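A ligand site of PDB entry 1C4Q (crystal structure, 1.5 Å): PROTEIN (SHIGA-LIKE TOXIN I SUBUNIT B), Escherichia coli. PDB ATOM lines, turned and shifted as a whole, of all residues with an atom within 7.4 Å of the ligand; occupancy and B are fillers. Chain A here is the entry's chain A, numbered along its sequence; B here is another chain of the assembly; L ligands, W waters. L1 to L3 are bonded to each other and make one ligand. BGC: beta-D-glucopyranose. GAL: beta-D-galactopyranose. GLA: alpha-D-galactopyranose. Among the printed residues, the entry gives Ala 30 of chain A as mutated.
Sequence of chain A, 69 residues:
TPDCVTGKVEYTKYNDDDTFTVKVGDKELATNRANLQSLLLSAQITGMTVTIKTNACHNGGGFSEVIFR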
ATOM      1  N   THR A   1      30.693 -10.370 -16.721  1.00  0.00           N
ATOM      2  CA  THR A   1      29.586  -9.432 -16.371  1.00  0.00           C
ATOM      3  C   THR A   1      28.515  -9.740 -17.381  1.00  0.00           C
ATOM      4  O   THR A   1      28.794  -9.839 -18.573  1.00  0.00           O
ATOM      5  CB  THR A   1      30.069  -7.993 -16.497  1.00  0.00           C
ATOM      6  OG1 THR A   1      31.287  -7.872 -15.746  1.00  0.00           O
ATOM      7  CG2 THR A   1      29.050  -6.993 -15.945  1.00  0.00           C
ATOM      8  N   PRO A   2      27.268  -9.891 -16.921  1.00  0.00           N
ATOM      9  CA  PRO A   2      26.141 -10.215 -17.810  1.00  0.00           C
ATOM     10  C   PRO A   2      25.687  -9.085 -18.752  1.00  0.00           C
ATOM     11  O   PRO A   2      25.797  -7.911 -18.431  1.00  0.00           O
ATOM     12  CB  PRO A   2      25.038 -10.601 -16.813  1.00  0.00           C
ATOM     13  CG  PRO A   2      25.298  -9.683 -15.645  1.00  0.00           C
ATOM     14  CD  PRO A   2      26.822  -9.739 -15.523  1.00  0.00           C
ATOM     15  N   THR A  19      28.963  12.472 -15.011  1.00  0.00           N
ATOM     16  CA  THR A  19      28.725  11.104 -15.514  1.00  0.00           C
ATOM     17  C   THR A  19      27.990  11.269 -16.842  1.00  0.00           C
ATOM     18  O   THR A  19      27.540  12.379 -17.171  1.00  0.00           O
ATOM     19  CB  THR A  19      27.903  10.232 -14.570  1.00  0.00           C
ATOM     20  OG1 THR A  19      26.621  10.796 -14.264  1.00  0.00           O
ATOM     21  CG2 THR A  19      28.717  10.019 -13.261  1.00  0.00           C
ATOM     22  N   PHE A  20      27.841  10.137 -17.547  1.00  0.00           N
ATOM     23  CA  PHE A  20      27.246  10.172 -18.904  1.00  0.00           C
ATOM     24  C   PHE A  20      26.202   9.080 -19.021  1.00  0.00           C
ATOM     25  O   PHE A  20      26.490   7.900 -18.800  1.00  0.00           O
ATOM     26  CB  PHE A  20      28.361   9.925 -19.912  1.00  0.00           C
ATOM     27  CG  PHE A  20      28.023  10.358 -21.337  1.00  0.00           C
ATOM     28  CD1 PHE A  20      27.951  11.698 -21.653  1.00  0.00           C
ATOM     29  CD2 PHE A  20      27.853   9.403 -22.348  1.00  0.00           C
ATOM     30  CE1 PHE A  20      27.715  12.111 -22.999  1.00  0.00           C
ATOM     31  CE2 PHE A  20      27.625   9.806 -23.676  1.00  0.00           C
ATOM     32  CZ  PHE A  20      27.560  11.140 -23.988  1.00  0.00           C
ATOM     33  N   ALA A  30      24.185   4.756 -16.780  1.00  0.00           N
ATOM     34  CA  ALA A  30      25.168   5.819 -16.727  1.00  0.00           C
ATOM     35  C   ALA A  30      26.546   5.358 -16.362  1.00  0.00           C
ATOM     36  O   ALA A  30      26.675   4.380 -15.610  1.00  0.00           O
ATOM     37  CB  ALA A  30      24.723   6.933 -15.738  1.00  0.00           C
ATOM     38  N   THR A  31      27.536   6.019 -16.876  1.00  0.00           N
ATOM     39  CA  THR A  31      28.913   5.657 -16.605  1.00  0.00           C
ATOM     40  C   THR A  31      29.723   6.819 -16.091  1.00  0.00           C
ATOM     41  O   THR A  31      29.517   7.967 -16.479  1.00  0.00           O
ATOM     42  CB  THR A  31      29.626   5.029 -17.848  1.00  0.00           C
ATOM     43  OG1 THR A  31      30.965   4.619 -17.535  1.00  0.00           O
ATOM     44  CG2 THR A  31      29.731   6.050 -18.960  1.00  0.00           C
ATOM     45  N   ASN A  32      30.650   6.514 -15.174  1.00  0.00           N
ATOM     46  CA  ASN A  32      31.545   7.527 -14.671  1.00  0.00           C
ATOM     47  C   ASN A  32      32.888   7.526 -15.363  1.00  0.00           C
ATOM     48  O   ASN A  32      33.816   8.262 -15.013  1.00  0.00           O
ATOM     49  CB  ASN A  32      31.723   7.337 -13.133  1.00  0.00           C
ATOM     50  CG  ASN A  32      32.495   6.078 -12.808  1.00  0.00           C
ATOM     51  OD1 ASN A  32      32.819   5.267 -13.698  1.00  0.00           O
ATOM     52  ND2 ASN A  32      32.795   5.873 -11.495  1.00  0.00           N
ATOM     53  N   ARG A  33      33.050   6.710 -16.432  1.00  0.00           N
ATOM     54  CA  ARG A  33      34.327   6.658 -17.104  1.00  0.00           C
ATOM     55  C   ARG A  33      34.394   7.749 -18.150  1.00  0.00           C
ATOM     56  O   ARG A  33      33.682   7.656 -19.177  1.00  0.00           O
ATOM     57  CB  ARG A  33      34.548   5.241 -17.736  1.00  0.00           C
ATOM     58  CG  ARG A  33      34.374   4.062 -16.730  1.00  0.00           C
ATOM     59  CD  ARG A  33      35.397   4.173 -15.598  1.00  0.00           C
ATOM     60  NE  ARG A  33      35.105   3.100 -14.638  1.00  0.00           N
ATOM     61  CZ  ARG A  33      35.628   1.863 -14.684  1.00  0.00           C
ATOM     62  NH1 ARG A  33      36.513   1.568 -15.622  1.00  0.00           N
ATOM     63  NH2 ARG A  33      35.188   0.910 -13.855  1.00  0.00           N
ATOM     64  N   LEU A  36      34.742   7.081 -22.031  1.00  0.00           N
ATOM     65  CA  LEU A  36      33.607   6.543 -22.768  1.00  0.00           C
ATOM     66  C   LEU A  36      32.708   7.576 -23.392  1.00  0.00           C
ATOM     67  O   LEU A  36      31.862   7.214 -24.230  1.00  0.00           O
ATOM     68  CB  LEU A  36      32.736   5.661 -21.888  1.00  0.00           C
ATOM     69  CG  LEU A  36      33.216   4.191 -21.734  1.00  0.00           C
ATOM     70  CD1 LEU A  36      32.286   3.447 -20.787  1.00  0.00           C
ATOM     71  CD2 LEU A  36      33.181   3.504 -23.176  1.00  0.00           C
ATOM     72  N   LYS A  53      27.161  -4.212 -20.630  1.00  0.00           N
ATOM     73  CA  LYS A  53      27.144  -5.297 -19.646  1.00  0.00           C
ATOM     74  C   LYS A  53      27.227  -4.649 -18.272  1.00  0.00           C
ATOM     75  O   LYS A  53      28.102  -3.842 -18.033  1.00  0.00           O
ATOM     76  CB  LYS A  53      28.354  -6.208 -19.811  1.00  0.00           C
ATOM     77  CG  LYS A  53      28.353  -7.002 -21.172  1.00  0.00           C
ATOM     78  CD  LYS A  53      29.694  -7.709 -21.369  1.00  0.00           C
ATOM     79  CE  LYS A  53      29.549  -9.037 -22.140  1.00  0.00           C
ATOM     80  NZ  LYS A  53      28.600  -9.994 -21.468  1.00  0.00           N
ATOM     81  N   THR A  54      26.330  -5.078 -17.384  1.00  0.00           N
ATOM     82  CA  THR A  54      26.345  -4.591 -16.001  1.00  0.00           C
ATOM     83  C   THR A  54      25.482  -5.450 -15.126  1.00  0.00           C
ATOM     84  O   THR A  54      24.499  -6.041 -15.570  1.00  0.00           O
ATOM     85  CB  THR A  54      25.836  -3.126 -15.898  1.00  0.00           C
ATOM     86  OG1 THR A  54      25.891  -2.681 -14.513  1.00  0.00           O
ATOM     87  CG2 THR A  54      24.452  -2.964 -16.486  1.00  0.00           C
ATOM     88  N   ASN A  55      25.864  -5.522 -13.850  1.00  0.00           N
ATOM     89  CA  ASN A  55      25.100  -6.252 -12.860  1.00  0.00           C
ATOM     90  C   ASN A  55      24.036  -5.301 -12.257  1.00  0.00           C
ATOM     91  O   ASN A  55      23.166  -5.765 -11.505  1.00  0.00           O
ATOM     92  CB  ASN A  55      26.032  -6.790 -11.731  1.00  0.00           C
ATOM     93  CG  ASN A  55      26.736  -8.096 -12.100  1.00  0.00           C
ATOM     94  OD1 ASN A  55      27.967  -8.226 -11.948  1.00  0.00           O
ATOM     95  ND2 ASN A  55      25.975  -9.058 -12.557  1.00  0.00           N
ATOM     96  N   ALA A  56      24.081  -3.999 -12.575  1.00  0.00           N
ATOM     97  CA  ALA A  56      23.067  -3.033 -12.085  1.00  0.00           C
ATOM     98  C   ALA A  56      22.173  -2.756 -13.297  1.00  0.00           C
ATOM     99  O   ALA A  56      22.135  -1.633 -13.824  1.00  0.00           O
ATOM    100  CB  ALA A  56      23.730  -1.777 -11.589  1.00  0.00           C
ATOM    101  N   CYS A  57      21.455  -3.806 -13.703  1.00  0.00           N
ATOM    102  CA  CYS A  57      20.605  -3.741 -14.875  1.00  0.00           C
ATOM    103  C   CYS A  57      19.198  -3.251 -14.571  1.00  0.00           C
ATOM    104  O   CYS A  57      18.226  -4.011 -14.524  1.00  0.00           O
ATOM    105  CB  CYS A  57      20.612  -5.097 -15.567  1.00  0.00           C
ATOM    106  SG  CYS A  57      19.929  -5.045 -17.285  1.00  0.00           S
ATOM    107  N   HIS A  58      19.125  -1.941 -14.356  1.00  0.00           N
ATOM    108  CA  HIS A  58      17.864  -1.292 -14.051  1.00  0.00           C
ATOM    109  C   HIS A  58      18.029   0.151 -14.490  1.00  0.00           C
ATOM    110  O   HIS A  58      19.131   0.609 -14.730  1.00  0.00           O
ATOM    111  CB  HIS A  58      17.521  -1.367 -12.529  1.00  0.00           C
ATOM    112  CG  HIS A  58      18.633  -0.936 -11.629  1.00  0.00           C
ATOM    113  ND1 HIS A  58      18.941   0.393 -11.405  1.00  0.00           N
ATOM    114  CD2 HIS A  58      19.533  -1.654 -10.923  1.00  0.00           C
ATOM    115  CE1 HIS A  58      20.008   0.467 -10.611  1.00  0.00           C
ATOM    116  NE2 HIS A  58      20.371  -0.768 -10.312  1.00  0.00           N
ATOM    117  N   GLY A  60      18.813   3.738 -14.655  1.00  0.00           N
ATOM    118  CA  GLY A  60      19.683   4.570 -13.845  1.00  0.00           C
ATOM    119  C   GLY A  60      20.889   3.806 -13.311  1.00  0.00           C
ATOM    120  O   GLY A  60      21.763   4.384 -12.648  1.00  0.00           O
ATOM    121  N   GLY A  61      20.961   2.528 -13.652  1.00  0.00           N
ATOM    122  CA  GLY A  61      22.088   1.697 -13.238  1.00  0.00           C
ATOM    123  C   GLY A  61      23.420   2.061 -13.815  1.00  0.00           C
ATOM    124  O   GLY A  61      23.511   2.665 -14.900  1.00  0.00           O
ATOM    125  N   GLY A  62      24.516   1.831 -13.077  1.00  0.00           N
ATOM    126  CA  GLY A  62      25.814   2.177 -13.607  1.00  0.00           C
ATOM    127  C   GLY A  62      26.479   1.085 -14.460  1.00  0.00           C
ATOM    128  O   GLY A  62      26.143  -0.062 -14.318  1.00  0.00           O
ATOM    129  N   PHE A  63      27.426   1.471 -15.299  1.00  0.00           N
ATOM    130  CA  PHE A  63      28.154   0.501 -16.116  1.00  0.00           C
ATOM    131  C   PHE A  63      29.490   1.029 -16.510  1.00  0.00           C
ATOM    132  O   PHE A  63      29.751   2.245 -16.436  1.00  0.00           O
ATOM    133  CB  PHE A  63      27.344   0.155 -17.409  1.00  0.00           C
ATOM    134  CG  PHE A  63      27.380   1.252 -18.466  1.00  0.00           C
ATOM    135  CD1 PHE A  63      26.467   2.281 -18.414  1.00  0.00           C
ATOM    136  CD2 PHE A  63      28.349   1.257 -19.451  1.00  0.00           C
ATOM    137  CE1 PHE A  63      26.521   3.351 -19.345  1.00  0.00           C
ATOM    138  CE2 PHE A  63      28.423   2.318 -20.380  1.00  0.00           C
ATOM    139  CZ  PHE A  63      27.492   3.372 -20.314  1.00  0.00           C
ATOM    140  N   SER A  64      30.400   0.102 -16.874  1.00  0.00           N
ATOM    141  CA  SER A  64      31.707   0.459 -17.383  1.00  0.00           C
ATOM    142  C   SER A  64      32.004  -0.363 -18.628  1.00  0.00           C
ATOM    143  O   SER A  64      32.862   0.058 -19.407  1.00  0.00           O
ATOM    144  CB  SER A  64      32.857   0.194 -16.376  1.00  0.00           C
ATOM    145  OG  SER A  64      32.803  -1.155 -15.994  1.00  0.00           O
ATOM    146  N   GLU A  65      31.289  -1.472 -18.819  1.00  0.00           N
ATOM    147  CA  GLU A  65      31.589  -2.349 -19.964  1.00  0.00           C
ATOM    148  C   GLU A  65      30.633  -2.170 -21.132  1.00  0.00           C
ATOM    149  O   GLU A  65      29.469  -2.308 -20.975  1.00  0.00           O
ATOM    150  CB  GLU A  65      31.583  -3.813 -19.528  1.00  0.00           C
ATOM    151  CG  GLU A  65      32.696  -4.117 -18.529  1.00  0.00           C
ATOM    152  CD  GLU A  65      32.655  -5.558 -18.081  1.00  0.00           C
ATOM    153  OE1 GLU A  65      32.752  -6.465 -18.954  1.00  0.00           O
ATOM    154  OE2 GLU A  65      32.470  -5.800 -16.871  1.00  0.00           O
ATOM    155  N   ASP B  16      36.193  -3.247 -17.614  1.00  0.00           N
ATOM    156  CA  ASP B  16      36.066  -2.626 -16.293  1.00  0.00           C
ATOM    157  C   ASP B  16      37.346  -2.034 -15.743  1.00  0.00           C
ATOM    158  O   ASP B  16      37.313  -1.119 -14.869  1.00  0.00           O
ATOM    159  CB  ASP B  16      35.476  -3.652 -15.333  1.00  0.00           C
ATOM    160  CG  ASP B  16      35.059  -3.034 -14.011  1.00  0.00           C
ATOM    161  OD1 ASP B  16      34.172  -2.155 -13.989  1.00  0.00           O
ATOM    162  OD2 ASP B  16      35.624  -3.465 -12.981  1.00  0.00           O
ATOM    163  N   ASP B  18      39.537  -0.438 -17.484  1.00  0.00           N
ATOM    164  CA  ASP B  18      39.949   0.583 -18.444  1.00  0.00           C
ATOM    165  C   ASP B  18      40.840   0.132 -19.570  1.00  0.00           C
ATOM    166  O   ASP B  18      41.401   0.957 -20.278  1.00  0.00           O
ATOM    167  CB  ASP B  18      40.502   1.845 -17.767  1.00  0.00           C
ATOM    168  CG  ASP B  18      39.512   2.440 -16.794  1.00  0.00           C
ATOM    169  OD1 ASP B  18      38.422   2.945 -17.197  1.00  0.00           O
ATOM    170  OD2 ASP B  18      39.824   2.375 -15.573  1.00  0.00           O
HETATM  171  C2  BGC L   1      28.505  -6.945  -7.825  1.00  0.00           C
HETATM  172  C3  BGC L   1      28.939  -5.489  -7.886  1.00  0.00           C
HETATM  173  C4  BGC L   1      27.744  -4.641  -8.327  1.00  0.00           C
HETATM  174  C5  BGC L   1      26.617  -4.862  -7.308  1.00  0.00           C
HETATM  175  C6  BGC L   1      25.380  -3.992  -7.487  1.00  0.00           C
HETATM  176  C1  BGC L   1      27.284  -7.120  -6.927  1.00  0.00           C
HETATM  177  O1  BGC L   1      26.804  -8.433  -7.016  1.00  0.00           O
HETATM  178  O2  BGC L   1      29.592  -7.726  -7.323  1.00  0.00           O
HETATM  179  O3  BGC L   1      30.026  -5.346  -8.792  1.00  0.00           O
HETATM  180  O4  BGC L   1      28.106  -3.258  -8.363  1.00  0.00           O
HETATM  181  O5  BGC L   1      26.210  -6.241  -7.345  1.00  0.00           O
HETATM  182  O6  BGC L   1      24.729  -4.271  -8.712  1.00  0.00           O
HETATM  183  C1  GAL L   2      27.686  -2.570  -9.510  1.00  0.00           C
HETATM  184  C2  GAL L   2      27.921  -1.074  -9.329  1.00  0.00           C
HETATM  185  C3  GAL L   2      27.522  -0.343 -10.621  1.00  0.00           C
HETATM  186  C4  GAL L   2      28.315  -0.923 -11.785  1.00  0.00           C
HETATM  187  C5  GAL L   2      28.081  -2.417 -11.863  1.00  0.00           C
HETATM  188  C6  GAL L   2      28.880  -3.138 -12.921  1.00  0.00           C
HETATM  189  O2  GAL L   2      27.113  -0.587  -8.261  1.00  0.00           O
HETATM  190  O3  GAL L   2      27.802   1.044 -10.478  1.00  0.00           O
HETATM  191  O4  GAL L   2      29.714  -0.645 -11.604  1.00  0.00           O
HETATM  192  O5  GAL L   2      28.465  -3.052 -10.612  1.00  0.00           O
HETATM  193  O6  GAL L   2      28.462  -4.491 -12.978  1.00  0.00           O
HETATM  194  C1  GLA L   3      30.416  -0.238 -12.762  1.00  0.00           C
HETATM  195  C2  GLA L   3      31.902  -0.256 -12.527  1.00  0.00           C
HETATM  196  C3  GLA L   3      32.266   0.821 -11.479  1.00  0.00           C
HETATM  197  C4  GLA L   3      31.775   2.183 -11.970  1.00  0.00           C
HETATM  198  C5  GLA L   3      30.275   2.121 -12.249  1.00  0.00           C
HETATM  199  C6  GLA L   3      29.617   3.405 -12.827  1.00  0.00           C
HETATM  200  O2  GLA L   3      32.305  -1.565 -12.100  1.00  0.00           O
HETATM  201  O3  GLA L   3      33.673   0.900 -11.335  1.00  0.00           O
HETATM  202  O4  GLA L   3      32.553   2.521 -13.125  1.00  0.00           O
HETATM  203  O5  GLA L   3      30.005   1.053 -13.196  1.00  0.00           O
HETATM  204  O6  GLA L   3      30.265   3.779 -14.043  1.00  0.00           O
HETATM  205  O   HOH W   1      28.586  -1.302  -5.665  1.00  0.00           O
HETATM  206  O   HOH W   2      31.459  -2.772  -9.866  1.00  0.00           O
HETATM  207  O   HOH W   3      35.319  -1.610 -10.998  1.00  0.00           O
HETATM  208  O   HOH W   4      34.629   3.529 -10.727  1.00  0.00           O
HETATM  209  O   HOH W   5      24.121  -0.238  -8.158  1.00  0.00           O
HETATM  210  O   HOH W   6      29.725  -2.561 -16.246  1.00  0.00           O
HETATM  211  O   HOH W   7      24.488   1.467 -10.251  1.00  0.00           O
HETATM  212  O   HOH W   8      29.710  -6.091 -11.365  1.00  0.00           O
HETATM  213  O   HOH W   9      31.020  -8.323  -4.764  1.00  0.00           O
HETATM  214  O   HOH W  10      29.873   1.794  -8.400  1.00  0.00           O
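The side-chain carboxylate of Asp 16 of chain B lies within salt-bridge range of the guanidinium group of Arg 33 (3.2 Å).
OG of Ser 64 lies within hydrogen-bond range of OD1 of Asp 16 of chain B (2.6 Å).
The backbone NH (N) of Phe 63 sits at hydrogen-bond distance from the backbone carbonyl oxygen (O) of Ala 30.
The side-chain hydroxyl (OG1) of Thr 31 sits at hydrogen-bond distance from the backbone carbonyl oxygen (O) of Phe 63, at 2.9 Å.
NE of Arg 33 lies within hydrogen-bond range of OD1 of Asn 32, at 3.3 Å.
The backbone NH (N) of Thr 54 lies within hydrogen-bond range of the backbone carbonyl oxygen (O) of Pro 2.
N of Arg 33 lies within hydrogen-bond range of OG1 of Thr 31 (3.2 Å).
O of Thr 1 lies within hydrogen-bond range of NZ of Lys 53, 2.9 Å away.
Thr 1 touches the ligand.
O of Ala 30 touches O6 of GLA L3 (3.96 Å).
CA of Thr 31 touches O6 of GLA L3, at 3.5 Å.
N of Ala 56 touches O6 of BGC L1 (3.9 Å).
O of Gly 62 touches C4 of GAL L2 (3.4 Å).
OG of Ser 64 touches C2 of GLA L3, 3.7 Å away.
12 residues have an atom within 4 Å of the ligand: Thr 1, Ala 30, Thr 31, Asn 32, Arg 33, Thr 54, Asn 55, Ala 56, Gly 62, Phe 63, Ser 64 and Asp 16 of chain B.
Water W8 bridges an oxygen (O6) of GAL L2 (2.6 Å) and the side-chain amide oxygen (OD1) of Asn 55 (2.8 Å).
Water W4 bridges an oxygen (O3) of GLA L3 and the side-chain amide nitrogen of Asn 32.
Water W3 lies within hydrogen-bond range of the side-chain carboxylate (OD2) of Asp 16 of chain B and an oxygen (O3) of GLA L3.
Water W7 lies within hydrogen-bond range of the backbone NH (N) of Gly 62 and an oxygen (O3) of GAL L2.
Water W6 lies within hydrogen-bond range of O of Lys 53 (2.7 Å), N of Ser 64 (2.8 Å) and N of Glu 65 (3.2 Å).
NH2 of Arg 33 lies within hydrogen-bond range of O3 of GLA L3, at 2.9 Å.
N of Phe 63 sits close to O5 of GLA L3, at 3.4 Å.
The backbone NH (N) of Asn 55 is in hydrogen-bond range of an oxygen (O6) of GAL L2, at 2.9 Å.
An oxygen (O6) of GLA L3 sits at hydrogen-bond distance from the backbone NH (N) of Asn 32, 3.0 Å away.
The side-chain amide oxygen of Asn 32 sits at hydrogen-bond distance from an oxygen (O4) of GLA L3 (2.8 Å).
O of Phe 63 sits at hydrogen-bond distance from O6 of GLA L3, at 2.9 Å.
OD1 of Asp 16 of chain B sits at hydrogen-bond distance from O2 of GLA L3, at 2.7 Å.
An oxygen (O6) of GAL L2 sits close to the side-chain hydroxyl (OG1) of Thr 54, 3.5 Å away.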
